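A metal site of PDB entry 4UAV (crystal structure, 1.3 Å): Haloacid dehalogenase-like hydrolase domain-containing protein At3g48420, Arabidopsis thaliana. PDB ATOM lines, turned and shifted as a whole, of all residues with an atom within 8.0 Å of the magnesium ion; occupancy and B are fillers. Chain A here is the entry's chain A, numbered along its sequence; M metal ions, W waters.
OD1 of Asp 9 is in salt-bridge range of NZ of Lys 160 (2.8 Å). The backbone carbonyl oxygen (O) of Val 183 sits at hydrogen-bond distance from the backbone NH (N) of Asp 9, 2.9 Å away. The side-chain sulfur of Cys 10 lies within hydrogen-bond range of the side-chain carboxylate of Asp 11 (3.6 Å). The side-chain hydroxyl (OG1) of Thr 17 is in hydrogen-bond range of the side-chain carboxylate (OD1) of Asp 11, at 2.7 Å. The side-chain carboxylate (OD2) of Asp 185 is in hydrogen-bond range of the side-chain hydroxyl (OG) of Ser 205 (2.7 Å). OG1 of Thr 208 is in hydrogen-bond range of O of Asp 185 (2.7 Å).
Of the 26 residues printed, 3 come within 4 Å of the magnesium ion.
The magnesium ion is bound by the side-chain carboxylate (OD2) of Asp 9 (2.0 Å), the backbone carbonyl oxygen (O) of Asp 11 (2.1 Å), water W2 (2.1 Å), water W3 (2.1 Å), the side-chain carboxylate (OD1) of Asp 185 (2.1 Å) and water W1 (2.1 Å).
Water W2 lies within hydrogen-bond range of OE2 of Glu 184 (2.7 Å) and OG of Ser 186 (2.9 Å).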
ATOM      1  N   PHE A   8     -14.027 -33.006  13.531  1.00  0.00           N
ATOM      2  CA  PHE A   8     -13.298 -31.782  13.696  1.00  0.00           C
ATOM      3  C   PHE A   8     -13.291 -30.994  12.416  1.00  0.00           C
ATOM      4  O   PHE A   8     -12.911 -31.506  11.360  1.00  0.00           O
ATOM      5  CB  PHE A   8     -11.833 -32.115  14.059  1.00  0.00           C
ATOM      6  CG  PHE A   8     -11.624 -32.728  15.423  1.00  0.00           C
ATOM      7  CD1 PHE A   8     -11.702 -34.101  15.580  1.00  0.00           C
ATOM      8  CD2 PHE A   8     -11.267 -31.925  16.503  1.00  0.00           C
ATOM      9  CE1 PHE A   8     -11.484 -34.642  16.806  1.00  0.00           C
ATOM     10  CE2 PHE A   8     -11.021 -32.450  17.771  1.00  0.00           C
ATOM     11  CZ  PHE A   8     -11.145 -33.881  17.855  1.00  0.00           C
ATOM     12  N   ASP A   9     -13.532 -29.676  12.538  1.00  0.00           N
ATOM     13  CA  ASP A   9     -13.074 -28.779  11.484  1.00  0.00           C
ATOM     14  C   ASP A   9     -11.527 -28.807  11.442  1.00  0.00           C
ATOM     15  O   ASP A   9     -10.905 -29.188  12.397  1.00  0.00           O
ATOM     16  CB  ASP A   9     -13.538 -27.370  11.757  1.00  0.00           C
ATOM     17  CG  ASP A   9     -13.155 -26.365  10.718  1.00  0.00           C
ATOM     18  OD1 ASP A   9     -13.213 -26.665   9.548  1.00  0.00           O
ATOM     19  OD2 ASP A   9     -12.868 -25.192  11.153  1.00  0.00           O
ATOM     20  N   CYS A  10     -10.959 -28.416  10.325  1.00  0.00           N
ATOM     21  CA  CYS A  10      -9.512 -28.284  10.202  1.00  0.00           C
ATOM     22  C   CYS A  10      -9.058 -26.837  10.654  1.00  0.00           C
ATOM     23  O   CYS A  10      -8.515 -26.734  11.734  1.00  0.00           O
ATOM     24  CB  CYS A  10      -8.993 -28.631   8.804  1.00  0.00           C
ATOM     25  SG  CYS A  10      -7.204 -28.537   8.665  1.00  0.00           S
ATOM     26  N   ASP A  11      -9.259 -25.839   9.816  1.00  0.00           N
ATOM     27  CA  ASP A  11      -8.717 -24.524  10.051  1.00  0.00           C
ATOM     28  C   ASP A  11      -9.367 -23.829  11.210  1.00  0.00           C
ATOM     29  O   ASP A  11     -10.574 -23.521  11.158  1.00  0.00           O
ATOM     30  CB  ASP A  11      -8.745 -23.677   8.796  1.00  0.00           C
ATOM     31  CG  ASP A  11      -7.853 -24.161   7.696  1.00  0.00           C
ATOM     32  OD1 ASP A  11      -6.933 -24.984   7.907  1.00  0.00           O
ATOM     33  OD2 ASP A  11      -8.010 -23.652   6.588  1.00  0.00           O
ATOM     34  N   GLY A  12      -8.565 -23.541  12.222  1.00  0.00           N
ATOM     35  CA  GLY A  12      -9.012 -22.905  13.446  1.00  0.00           C
ATOM     36  C   GLY A  12      -9.351 -23.850  14.549  1.00  0.00           C
ATOM     37  O   GLY A  12      -9.654 -23.447  15.664  1.00  0.00           O
ATOM     38  N   VAL A  13      -9.358 -25.183  14.241  1.00  0.00           N
ATOM     39  CA  VAL A  13      -9.680 -26.209  15.231  1.00  0.00           C
ATOM     40  C   VAL A  13      -8.447 -27.094  15.445  1.00  0.00           C
ATOM     41  O   VAL A  13      -7.939 -27.182  16.544  1.00  0.00           O
ATOM     42  CB  VAL A  13     -10.937 -26.956  14.902  1.00  0.00           C
ATOM     43  CG1 VAL A  13     -11.146 -28.189  15.776  1.00  0.00           C
ATOM     44  CG2 VAL A  13     -12.165 -26.039  14.995  1.00  0.00           C
ATOM     45  N   LEU A  14      -7.996 -27.791  14.424  1.00  0.00           N
ATOM     46  CA  LEU A  14      -6.809 -28.628  14.597  1.00  0.00           C
ATOM     47  C   LEU A  14      -5.533 -27.786  14.783  1.00  0.00           C
ATOM     48  O   LEU A  14      -4.683 -28.106  15.570  1.00  0.00           O
ATOM     49  CB  LEU A  14      -6.570 -29.571  13.416  1.00  0.00           C
ATOM     50  CG  LEU A  14      -7.704 -30.585  13.099  1.00  0.00           C
ATOM     51  CD1 LEU A  14      -7.300 -31.372  11.834  1.00  0.00           C
ATOM     52  CD2 LEU A  14      -7.962 -31.522  14.256  1.00  0.00           C
ATOM     53  N   VAL A  15      -5.476 -26.704  14.003  1.00  0.00           N
ATOM     54  CA  VAL A  15      -4.370 -25.764  13.951  1.00  0.00           C
ATOM     55  C   VAL A  15      -5.015 -24.384  13.787  1.00  0.00           C
ATOM     56  O   VAL A  15      -6.054 -24.250  13.120  1.00  0.00           O
ATOM     57  CB  VAL A  15      -3.417 -26.044  12.747  1.00  0.00           C
ATOM     58  CG1 VAL A  15      -2.725 -27.411  12.886  1.00  0.00           C
ATOM     59  CG2 VAL A  15      -4.128 -26.098  11.455  1.00  0.00           C
ATOM     60  N   THR A  17      -4.716 -22.081  11.647  1.00  0.00           N
ATOM     61  CA  THR A  17      -4.070 -22.067  10.365  1.00  0.00           C
ATOM     62  C   THR A  17      -3.737 -20.617   9.913  1.00  0.00           C
ATOM     63  O   THR A  17      -2.634 -20.378   9.371  1.00  0.00           O
ATOM     64  CB  THR A  17      -4.921 -22.769   9.282  1.00  0.00           C
ATOM     65  OG1 THR A  17      -5.376 -23.981   9.852  1.00  0.00           O
ATOM     66  CG2 THR A  17      -4.116 -23.013   8.040  1.00  0.00           C
ATOM     67  N   CYS A 124     -13.595 -32.480   8.771  1.00  0.00           N
ATOM     68  CA  CYS A 124     -14.596 -31.917   7.820  1.00  0.00           C
ATOM     69  C   CYS A 124     -14.262 -30.462   7.486  1.00  0.00           C
ATOM     70  O   CYS A 124     -14.371 -29.593   8.388  1.00  0.00           O
ATOM     71  CB  CYS A 124     -15.999 -31.961   8.399  1.00  0.00           C
ATOM     72  SG  CYS A 124     -16.529 -33.628   8.592  1.00  0.00           S
ATOM     73  N   SER A 125     -13.806 -30.123   6.265  1.00  0.00           N
ATOM     74  CA  SER A 125     -13.222 -28.831   5.943  1.00  0.00           C
ATOM     75  C   SER A 125     -13.624 -28.404   4.563  1.00  0.00           C
ATOM     76  O   SER A 125     -13.820 -29.205   3.701  1.00  0.00           O
ATOM     77  CB  SER A 125     -11.701 -28.951   6.004  1.00  0.00           C
ATOM     78  OG  SER A 125     -11.043 -27.710   5.654  1.00  0.00           O
ATOM     79  N   THR A 126     -13.683 -27.103   4.341  1.00  0.00           N
ATOM     80  CA  THR A 126     -13.772 -26.493   3.020  1.00  0.00           C
ATOM     81  C   THR A 126     -12.382 -26.312   2.337  1.00  0.00           C
ATOM     82  O   THR A 126     -12.335 -25.922   1.147  1.00  0.00           O
ATOM     83  CB  THR A 126     -14.505 -25.143   3.053  1.00  0.00           C
ATOM     84  OG1 THR A 126     -13.674 -24.180   3.734  1.00  0.00           O
ATOM     85  CG2 THR A 126     -15.891 -25.265   3.573  1.00  0.00           C
ATOM     86  N   LYS A 160     -19.876 -25.275   3.635  1.00  0.00           N
ATOM     87  CA  LYS A 160     -20.419 -24.656   4.837  1.00  0.00           C
ATOM     88  C   LYS A 160     -20.800 -23.187   4.541  1.00  0.00           C
ATOM     89  O   LYS A 160     -20.023 -22.524   3.849  1.00  0.00           O
ATOM     90  CB  LYS A 160     -19.319 -24.687   5.942  1.00  0.00           C
ATOM     91  CG  LYS A 160     -18.820 -26.059   6.366  1.00  0.00           C
ATOM     92  CD  LYS A 160     -17.757 -25.991   7.466  1.00  0.00           C
ATOM     93  CE  LYS A 160     -16.945 -27.238   7.623  1.00  0.00           C
ATOM     94  NZ  LYS A 160     -15.816 -27.013   8.603  1.00  0.00           N
ATOM     95  N   TYR A 166     -20.855 -32.409   6.754  1.00  0.00           N
ATOM     96  CA  TYR A 166     -21.107 -33.100   8.000  1.00  0.00           C
ATOM     97  C   TYR A 166     -22.018 -34.339   7.733  1.00  0.00           C
ATOM     98  O   TYR A 166     -21.815 -35.416   8.311  1.00  0.00           O
ATOM     99  CB  TYR A 166     -21.578 -32.179   9.085  1.00  0.00           C
ATOM    100  CG  TYR A 166     -20.479 -31.299   9.577  1.00  0.00           C
ATOM    101  CD1 TYR A 166     -19.388 -31.835  10.171  1.00  0.00           C
ATOM    102  CD2 TYR A 166     -20.558 -29.940   9.515  1.00  0.00           C
ATOM    103  CE1 TYR A 166     -18.363 -31.036  10.608  1.00  0.00           C
ATOM    104  CE2 TYR A 166     -19.514 -29.102   9.993  1.00  0.00           C
ATOM    105  CZ  TYR A 166     -18.392 -29.673  10.485  1.00  0.00           C
ATOM    106  OH  TYR A 166     -17.345 -28.969  10.951  1.00  0.00           O
ATOM    107  N   VAL A 183     -16.509 -30.262  16.490  1.00  0.00           N
ATOM    108  CA  VAL A 183     -15.722 -29.157  17.064  1.00  0.00           C
ATOM    109  C   VAL A 183     -15.413 -28.216  15.911  1.00  0.00           C
ATOM    110  O   VAL A 183     -14.746 -28.527  14.935  1.00  0.00           O
ATOM    111  CB  VAL A 183     -14.374 -29.687  17.734  1.00  0.00           C
ATOM    112  CG1 VAL A 183     -13.708 -28.506  18.405  1.00  0.00           C
ATOM    113  CG2 VAL A 183     -14.692 -30.825  18.708  1.00  0.00           C
ATOM    114  N   GLU A 184     -15.925 -26.966  16.066  1.00  0.00           N
ATOM    115  CA  GLU A 184     -15.858 -25.911  15.064  1.00  0.00           C
ATOM    116  C   GLU A 184     -15.252 -24.627  15.725  1.00  0.00           C
ATOM    117  O   GLU A 184     -15.216 -24.513  16.925  1.00  0.00           O
ATOM    118  CB  GLU A 184     -17.284 -25.590  14.521  1.00  0.00           C
ATOM    119  CG  GLU A 184     -17.572 -26.318  13.241  1.00  0.00           C
ATOM    120  CD  GLU A 184     -16.836 -25.775  12.059  1.00  0.00           C
ATOM    121  OE1 GLU A 184     -16.993 -26.364  10.972  1.00  0.00           O
ATOM    122  OE2 GLU A 184     -16.139 -24.753  12.207  1.00  0.00           O
ATOM    123  N   ASP A 185     -14.799 -23.681  14.858  1.00  0.00           N
ATOM    124  CA  ASP A 185     -14.332 -22.411  15.368  1.00  0.00           C
ATOM    125  C   ASP A 185     -15.085 -21.238  14.816  1.00  0.00           C
ATOM    126  O   ASP A 185     -14.790 -20.114  15.307  1.00  0.00           O
ATOM    127  CB  ASP A 185     -12.828 -22.206  15.089  1.00  0.00           C
ATOM    128  CG  ASP A 185     -12.476 -22.026  13.663  1.00  0.00           C
ATOM    129  OD1 ASP A 185     -12.936 -22.897  12.876  1.00  0.00           O
ATOM    130  OD2 ASP A 185     -11.828 -21.047  13.316  1.00  0.00           O
ATOM    131  N   SER A 186     -15.986 -21.348  13.835  1.00  0.00           N
ATOM    132  CA  SER A 186     -16.595 -20.201  13.187  1.00  0.00           C
ATOM    133  C   SER A 186     -18.088 -20.311  13.218  1.00  0.00           C
ATOM    134  O   SER A 186     -18.633 -21.447  13.328  1.00  0.00           O
ATOM    135  CB  SER A 186     -16.108 -20.028  11.779  1.00  0.00           C
ATOM    136  OG  SER A 186     -16.616 -21.064  10.926  1.00  0.00           O
ATOM    137  N   ALA A 187     -18.767 -19.165  13.145  1.00  0.00           N
ATOM    138  CA  ALA A 187     -20.221 -19.163  13.142  1.00  0.00           C
ATOM    139  C   ALA A 187     -20.771 -19.955  11.949  1.00  0.00           C
ATOM    140  O   ALA A 187     -21.791 -20.590  12.074  1.00  0.00           O
ATOM    141  CB  ALA A 187     -20.768 -17.707  13.114  1.00  0.00           C
ATOM    142  N   ILE A 188     -20.179 -19.771  10.783  1.00  0.00           N
ATOM    143  CA  ILE A 188     -20.669 -20.477   9.564  1.00  0.00           C
ATOM    144  C   ILE A 188     -20.415 -21.994   9.675  1.00  0.00           C
ATOM    145  O   ILE A 188     -21.257 -22.777   9.234  1.00  0.00           O
ATOM    146  CB  ILE A 188     -20.092 -19.839   8.323  1.00  0.00           C
ATOM    147  CG1 ILE A 188     -21.109 -18.851   7.702  1.00  0.00           C
ATOM    148  CG2 ILE A 188     -19.811 -20.830   7.215  1.00  0.00           C
ATOM    149  CD1 ILE A 188     -21.625 -17.850   8.576  1.00  0.00           C
ATOM    150  N   GLY A 189     -19.291 -22.387  10.308  1.00  0.00           N
ATOM    151  CA  GLY A 189     -19.085 -23.821  10.474  1.00  0.00           C
ATOM    152  C   GLY A 189     -20.083 -24.386  11.501  1.00  0.00           C
ATOM    153  O   GLY A 189     -20.597 -25.511  11.322  1.00  0.00           O
ATOM    154  N   LEU A 190     -20.317 -23.666  12.588  1.00  0.00           N
ATOM    155  CA  LEU A 190     -21.337 -24.013  13.561  1.00  0.00           C
ATOM    156  C   LEU A 190     -22.675 -24.161  12.874  1.00  0.00           C
ATOM    157  O   LEU A 190     -23.388 -25.142  13.146  1.00  0.00           O
ATOM    158  CB  LEU A 190     -21.377 -22.918  14.630  1.00  0.00           C
ATOM    159  CG  LEU A 190     -22.583 -22.920  15.562  1.00  0.00           C
ATOM    160  CD1 LEU A 190     -22.643 -24.198  16.365  1.00  0.00           C
ATOM    161  CD2 LEU A 190     -22.568 -21.639  16.384  1.00  0.00           C
ATOM    162  N   THR A 203     -14.499 -23.997  19.629  1.00  0.00           N
ATOM    163  CA  THR A 203     -13.215 -23.559  20.172  1.00  0.00           C
ATOM    164  C   THR A 203     -12.833 -22.368  19.311  1.00  0.00           C
ATOM    165  O   THR A 203     -12.394 -22.449  18.202  1.00  0.00           O
ATOM    166  CB  THR A 203     -12.124 -24.635  20.094  1.00  0.00           C
ATOM    167  OG1 THR A 203     -11.905 -25.085  18.744  1.00  0.00           O
ATOM    168  CG2 THR A 203     -12.494 -25.809  20.959  1.00  0.00           C
ATOM    169  N   SER A 205     -11.003 -19.374  17.563  1.00  0.00           N
ATOM    170  CA  SER A 205      -9.629 -19.280  17.036  1.00  0.00           C
ATOM    171  C   SER A 205      -9.189 -17.843  16.902  1.00  0.00           C
ATOM    172  O   SER A 205      -9.893 -16.935  17.309  1.00  0.00           O
ATOM    173  CB  SER A 205      -9.557 -20.038  15.676  1.00  0.00           C
ATOM    174  OG  SER A 205     -10.266 -19.376  14.687  1.00  0.00           O
ATOM    175  N   THR A 208     -11.799 -15.533  15.087  1.00  0.00           N
ATOM    176  CA  THR A 208     -13.216 -15.840  15.192  1.00  0.00           C
ATOM    177  C   THR A 208     -13.840 -15.538  16.529  1.00  0.00           C
ATOM    178  O   THR A 208     -14.990 -15.802  16.752  1.00  0.00           O
ATOM    179  CB  THR A 208     -13.570 -17.302  14.793  1.00  0.00           C
ATOM    180  OG1 THR A 208     -13.115 -18.136  15.875  1.00  0.00           O
ATOM    181  CG2 THR A 208     -13.004 -17.684  13.493  1.00  0.00           C
ATOM    182  N   GLU A 211     -17.291 -13.795  16.734  1.00  0.00           N
ATOM    183  CA  GLU A 211     -18.395 -14.299  15.905  1.00  0.00           C
ATOM    184  C   GLU A 211     -19.588 -14.737  16.782  1.00  0.00           C
ATOM    185  O   GLU A 211     -19.507 -14.864  18.003  1.00  0.00           O
ATOM    186  CB  GLU A 211     -17.895 -15.427  14.973  1.00  0.00           C
ATOM    187  CG  GLU A 211     -16.948 -14.879  13.949  1.00  0.00           C
ATOM    188  CD  GLU A 211     -16.501 -15.843  12.908  1.00  0.00           C
ATOM    189  OE1 GLU A 211     -17.062 -16.955  12.804  1.00  0.00           O
ATOM    190  OE2 GLU A 211     -15.558 -15.508  12.136  1.00  0.00           O
HETATM  191 MG    MG M   1     -12.625 -23.258  10.828  1.00  0.00          MG
HETATM  192  O   HOH W   1     -12.170 -21.170  10.687  1.00  0.00           O
HETATM  193  O   HOH W   2     -14.705 -23.160  10.598  1.00  0.00           O
HETATM  194  O   HOH W   3     -12.461 -23.298   8.736  1.00  0.00           O
